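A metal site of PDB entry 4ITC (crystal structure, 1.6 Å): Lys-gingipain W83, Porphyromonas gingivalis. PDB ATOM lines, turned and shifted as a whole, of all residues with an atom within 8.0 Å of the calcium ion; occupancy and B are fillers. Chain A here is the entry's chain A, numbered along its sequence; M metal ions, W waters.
The side-chain carboxylate (OD1) of Asp 22 sits close to the backbone NH (N) of Asp 61, 2.8 Å away.
The backbone NH (N) of Gly 25 sits at hydrogen-bond distance from the side-chain carboxylate (OD2) of Asp 20, at 2.8 Å.
The backbone carbonyl oxygen of Asn 62 is in hydrogen-bond range of the indole nitrogen of Trp 28 (3.0 Å).
The backbone NH (N) of His 153 lies within hydrogen-bond range of the backbone carbonyl oxygen (O) of Asn 62 (2.8 Å).
The side-chain amide nitrogen (ND2) of Asn 62 is in hydrogen-bond range of the side-chain hydroxyl (OG) of Ser 47, 2.8 Å away.
The side-chain carboxylate (OD1) of Asp 20 lies close to the backbone NH (N) of Gly 23, at 3.2 Å.
Of the 19 residues printed, 5 come within 4 Å of the calcium ion.
The nearest printed residue that does not touch the calcium ion is Pro 60 (4.4 Å).
The calcium ion is bound by the side-chain carboxylate (OD1) of Asp 20, the backbone carbonyl oxygen (O) of His 26, the side-chain carboxylate (OD1) of Asp 22, the side-chain amide oxygen (OD1) of Asn 62, the side-chain carboxylate (OD1) of Asp 24, water W1 and the side-chain carboxylate (OD2) of Asp 22.
The calcium ion has seven donor atoms within binding distance.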
ATOM      1  N   ILE A  19       6.175  11.991 -13.081  1.00  0.00           N
ATOM      2  CA  ILE A  19       6.701  10.959 -12.191  1.00  0.00           C
ATOM      3  C   ILE A  19       5.543  10.233 -11.526  1.00  0.00           C
ATOM      4  O   ILE A  19       4.773  10.807 -10.791  1.00  0.00           O
ATOM      5  CB  ILE A  19       7.648  11.469 -11.102  1.00  0.00           C
ATOM      6  CG1 ILE A  19       8.717  12.414 -11.696  1.00  0.00           C
ATOM      7  CG2 ILE A  19       8.250  10.287 -10.382  1.00  0.00           C
ATOM      8  CD1 ILE A  19       9.556  13.084 -10.626  1.00  0.00           C
ATOM      9  N   ASP A  20       5.481   8.932 -11.780  1.00  0.00           N
ATOM     10  CA  ASP A  20       4.547   8.050 -11.115  1.00  0.00           C
ATOM     11  C   ASP A  20       5.275   7.476  -9.930  1.00  0.00           C
ATOM     12  O   ASP A  20       5.835   6.337  -9.980  1.00  0.00           O
ATOM     13  CB  ASP A  20       4.125   6.941 -12.079  1.00  0.00           C
ATOM     14  CG  ASP A  20       3.344   5.833 -11.429  1.00  0.00           C
ATOM     15  OD1 ASP A  20       2.711   6.024 -10.386  1.00  0.00           O
ATOM     16  OD2 ASP A  20       3.355   4.698 -12.015  1.00  0.00           O
ATOM     17  N   ALA A  21       5.330   8.221  -8.828  1.00  0.00           N
ATOM     18  CA  ALA A  21       6.241   7.862  -7.758  1.00  0.00           C
ATOM     19  C   ALA A  21       5.803   6.635  -6.979  1.00  0.00           C
ATOM     20  O   ALA A  21       6.638   5.879  -6.466  1.00  0.00           O
ATOM     21  CB  ALA A  21       6.490   9.033  -6.837  1.00  0.00           C
ATOM     22  N   ASP A  22       4.497   6.412  -6.917  1.00  0.00           N
ATOM     23  CA  ASP A  22       3.954   5.260  -6.182  1.00  0.00           C
ATOM     24  C   ASP A  22       4.083   3.969  -7.027  1.00  0.00           C
ATOM     25  O   ASP A  22       4.038   2.876  -6.431  1.00  0.00           O
ATOM     26  CB  ASP A  22       2.521   5.498  -5.823  1.00  0.00           C
ATOM     27  CG  ASP A  22       1.681   5.737  -7.040  1.00  0.00           C
ATOM     28  OD1 ASP A  22       1.692   6.904  -7.523  1.00  0.00           O
ATOM     29  OD2 ASP A  22       1.035   4.781  -7.547  1.00  0.00           O
ATOM     30  N   GLY A  23       4.277   4.085  -8.341  1.00  0.00           N
ATOM     31  CA  GLY A  23       4.630   2.943  -9.221  1.00  0.00           C
ATOM     32  C   GLY A  23       3.451   2.099  -9.709  1.00  0.00           C
ATOM     33  O   GLY A  23       3.644   1.006 -10.250  1.00  0.00           O
ATOM     34  N   ASP A  24       2.222   2.594  -9.587  1.00  0.00           N
ATOM     35  CA  ASP A  24       1.036   1.787 -10.024  1.00  0.00           C
ATOM     36  C   ASP A  24       0.741   1.829 -11.513  1.00  0.00           C
ATOM     37  O   ASP A  24      -0.192   1.175 -11.988  1.00  0.00           O
ATOM     38  CB  ASP A  24      -0.206   2.137  -9.178  1.00  0.00           C
ATOM     39  CG  ASP A  24      -0.774   3.557  -9.441  1.00  0.00           C
ATOM     40  OD1 ASP A  24      -0.120   4.317 -10.192  1.00  0.00           O
ATOM     41  OD2 ASP A  24      -1.815   3.851  -8.868  1.00  0.00           O
ATOM     42  N   GLY A  25       1.484   2.633 -12.258  1.00  0.00           N
ATOM     43  CA  GLY A  25       1.268   2.753 -13.669  1.00  0.00           C
ATOM     44  C   GLY A  25       0.252   3.803 -14.090  1.00  0.00           C
ATOM     45  O   GLY A  25      -0.110   3.909 -15.271  1.00  0.00           O
ATOM     46  N   HIS A  26      -0.266   4.527 -13.095  1.00  0.00           N
ATOM     47  CA  HIS A  26      -1.238   5.594 -13.308  1.00  0.00           C
ATOM     48  C   HIS A  26      -0.629   6.907 -12.865  1.00  0.00           C
ATOM     49  O   HIS A  26      -0.205   7.027 -11.735  1.00  0.00           O
ATOM     50  CB  HIS A  26      -2.506   5.349 -12.482  1.00  0.00           C
ATOM     51  CG  HIS A  26      -3.181   4.082 -12.795  1.00  0.00           C
ATOM     52  ND1 HIS A  26      -4.139   3.973 -13.780  1.00  0.00           N
ATOM     53  CD2 HIS A  26      -3.085   2.861 -12.233  1.00  0.00           C
ATOM     54  CE1 HIS A  26      -4.549   2.718 -13.845  1.00  0.00           C
ATOM     55  NE2 HIS A  26      -3.931   2.032 -12.907  1.00  0.00           N
ATOM     56  N   GLY A  27      -0.554   7.882 -13.766  1.00  0.00           N
ATOM     57  CA  GLY A  27       0.001   9.200 -13.438  1.00  0.00           C
ATOM     58  C   GLY A  27      -0.924  10.291 -13.933  1.00  0.00           C
ATOM     59  O   GLY A  27      -2.086  10.063 -14.293  1.00  0.00           O
ATOM     60  N   TRP A  28      -0.348  11.486 -14.037  1.00  0.00           N
ATOM     61  CA  TRP A  28      -1.077  12.607 -14.652  1.00  0.00           C
ATOM     62  C   TRP A  28      -1.279  12.280 -16.133  1.00  0.00           C
ATOM     63  O   TRP A  28      -0.348  11.780 -16.798  1.00  0.00           O
ATOM     64  CB  TRP A  28      -0.293  13.922 -14.528  1.00  0.00           C
ATOM     65  CG  TRP A  28      -0.300  14.500 -13.138  1.00  0.00           C
ATOM     66  CD1 TRP A  28       0.628  14.312 -12.137  1.00  0.00           C
ATOM     67  CD2 TRP A  28      -1.284  15.376 -12.607  1.00  0.00           C
ATOM     68  NE1 TRP A  28       0.254  14.997 -11.017  1.00  0.00           N
ATOM     69  CE2 TRP A  28      -0.915  15.688 -11.288  1.00  0.00           C
ATOM     70  CE3 TRP A  28      -2.467  15.924 -13.122  1.00  0.00           C
ATOM     71  CZ2 TRP A  28      -1.660  16.526 -10.471  1.00  0.00           C
ATOM     72  CZ3 TRP A  28      -3.216  16.762 -12.334  1.00  0.00           C
ATOM     73  CH2 TRP A  28      -2.825  17.051 -10.996  1.00  0.00           C
ATOM     74  N   SER A  47      -5.453  13.536 -12.687  1.00  0.00           N
ATOM     75  CA  SER A  47      -4.826  12.445 -11.974  1.00  0.00           C
ATOM     76  C   SER A  47      -5.893  11.782 -11.110  1.00  0.00           C
ATOM     77  O   SER A  47      -6.770  12.427 -10.526  1.00  0.00           O
ATOM     78  CB  SER A  47      -3.681  12.973 -11.127  1.00  0.00           C
ATOM     79  OG  SER A  47      -3.086  11.974 -10.344  1.00  0.00           O
ATOM     80  N   GLU A  48      -5.824  10.442 -11.039  1.00  0.00           N
ATOM     81  CA  GLU A  48      -6.856   9.595 -10.454  1.00  0.00           C
ATOM     82  C   GLU A  48      -6.553   9.137  -9.027  1.00  0.00           C
ATOM     83  O   GLU A  48      -5.475   8.578  -8.749  1.00  0.00           O
ATOM     84  CB  GLU A  48      -7.000   8.337 -11.311  1.00  0.00           C
ATOM     85  CG  GLU A  48      -7.418   8.615 -12.744  1.00  0.00           C
ATOM     86  CD  GLU A  48      -7.047   7.487 -13.684  1.00  0.00           C
ATOM     87  OE1 GLU A  48      -8.009   6.930 -14.281  1.00  0.00           O
ATOM     88  OE2 GLU A  48      -5.836   7.139 -13.793  1.00  0.00           O
ATOM     89  N   LEU A  58      -7.155   3.897  -5.879  1.00  0.00           N
ATOM     90  CA  LEU A  58      -5.722   4.103  -6.041  1.00  0.00           C
ATOM     91  C   LEU A  58      -5.153   4.911  -4.895  1.00  0.00           C
ATOM     92  O   LEU A  58      -5.906   5.573  -4.174  1.00  0.00           O
ATOM     93  CB  LEU A  58      -5.473   4.829  -7.359  1.00  0.00           C
ATOM     94  CG  LEU A  58      -6.036   4.119  -8.575  1.00  0.00           C
ATOM     95  CD1 LEU A  58      -5.888   4.980  -9.814  1.00  0.00           C
ATOM     96  CD2 LEU A  58      -5.286   2.805  -8.749  1.00  0.00           C
ATOM     97  N   THR A  59      -3.833   4.842  -4.724  1.00  0.00           N
ATOM     98  CA  THR A  59      -3.104   5.657  -3.773  1.00  0.00           C
ATOM     99  C   THR A  59      -1.993   6.478  -4.510  1.00  0.00           C
ATOM    100  O   THR A  59      -0.778   6.201  -4.361  1.00  0.00           O
ATOM    101  CB  THR A  59      -2.537   4.815  -2.627  1.00  0.00           C
ATOM    102  OG1 THR A  59      -1.673   3.813  -3.170  1.00  0.00           O
ATOM    103  CG2 THR A  59      -3.651   4.189  -1.807  1.00  0.00           C
ATOM    104  N   PRO A  60      -2.416   7.505  -5.261  1.00  0.00           N
ATOM    105  CA  PRO A  60      -1.450   8.249  -6.083  1.00  0.00           C
ATOM    106  C   PRO A  60      -0.350   8.949  -5.284  1.00  0.00           C
ATOM    107  O   PRO A  60      -0.599   9.462  -4.175  1.00  0.00           O
ATOM    108  CB  PRO A  60      -2.300   9.306  -6.801  1.00  0.00           C
ATOM    109  CG  PRO A  60      -3.548   9.376  -6.004  1.00  0.00           C
ATOM    110  CD  PRO A  60      -3.780   7.994  -5.488  1.00  0.00           C
ATOM    111  N   ASP A  61       0.823   9.015  -5.890  1.00  0.00           N
ATOM    112  CA  ASP A  61       1.847   9.962  -5.560  1.00  0.00           C
ATOM    113  C   ASP A  61       2.452  10.343  -6.906  1.00  0.00           C
ATOM    114  O   ASP A  61       3.501   9.828  -7.336  1.00  0.00           O
ATOM    115  CB  ASP A  61       2.850   9.387  -4.584  1.00  0.00           C
ATOM    116  CG  ASP A  61       3.878  10.407  -4.153  1.00  0.00           C
ATOM    117  OD1 ASP A  61       3.727  11.585  -4.526  1.00  0.00           O
ATOM    118  OD2 ASP A  61       4.871  10.018  -3.456  1.00  0.00           O
ATOM    119  N   ASN A  62       1.722  11.234  -7.599  1.00  0.00           N
ATOM    120  CA  ASN A  62       2.000  11.536  -9.031  1.00  0.00           C
ATOM    121  C   ASN A  62       2.437  12.980  -9.178  1.00  0.00           C
ATOM    122  O   ASN A  62       1.731  13.897  -8.677  1.00  0.00           O
ATOM    123  CB  ASN A  62       0.773  11.339  -9.896  1.00  0.00           C
ATOM    124  CG  ASN A  62       0.115   9.945  -9.794  1.00  0.00           C
ATOM    125  OD1 ASN A  62       0.771   8.904  -9.496  1.00  0.00           O
ATOM    126  ND2 ASN A  62      -1.195   9.900 -10.140  1.00  0.00           N
ATOM    127  N   TYR A  63       3.492  13.201  -9.931  1.00  0.00           N
ATOM    128  CA  TYR A  63       4.073  14.521 -10.146  1.00  0.00           C
ATOM    129  C   TYR A  63       3.952  14.903 -11.582  1.00  0.00           C
ATOM    130  O   TYR A  63       4.168  14.087 -12.482  1.00  0.00           O
ATOM    131  CB  TYR A  63       5.551  14.562  -9.812  1.00  0.00           C
ATOM    132  CG  TYR A  63       5.946  14.337  -8.346  1.00  0.00           C
ATOM    133  CD1 TYR A  63       5.892  13.105  -7.753  1.00  0.00           C
ATOM    134  CD2 TYR A  63       6.433  15.384  -7.598  1.00  0.00           C
ATOM    135  CE1 TYR A  63       6.274  12.921  -6.448  1.00  0.00           C
ATOM    136  CE2 TYR A  63       6.841  15.213  -6.296  1.00  0.00           C
ATOM    137  CZ  TYR A  63       6.766  13.952  -5.743  1.00  0.00           C
ATOM    138  OH  TYR A  63       7.192  13.757  -4.451  1.00  0.00           O
ATOM    139  N   HIS A 153      -0.056  15.102  -6.823  1.00  0.00           N
ATOM    140  CA  HIS A 153      -1.311  14.487  -6.321  1.00  0.00           C
ATOM    141  C   HIS A 153      -0.938  13.354  -5.417  1.00  0.00           C
ATOM    142  O   HIS A 153      -0.357  12.393  -5.870  1.00  0.00           O
ATOM    143  CB  HIS A 153      -2.130  13.992  -7.495  1.00  0.00           C
ATOM    144  CG  HIS A 153      -3.461  13.439  -7.126  1.00  0.00           C
ATOM    145  ND1 HIS A 153      -4.138  12.536  -7.920  1.00  0.00           N
ATOM    146  CD2 HIS A 153      -4.297  13.756  -6.120  1.00  0.00           C
ATOM    147  CE1 HIS A 153      -5.319  12.281  -7.389  1.00  0.00           C
ATOM    148  NE2 HIS A 153      -5.430  13.010  -6.283  1.00  0.00           N
HETATM  149 CA    CA M   1       0.612   6.523  -9.619  1.00  0.00          CA
HETATM  150  O   HOH W   1      -1.678   6.471  -8.787  1.00  0.00           O
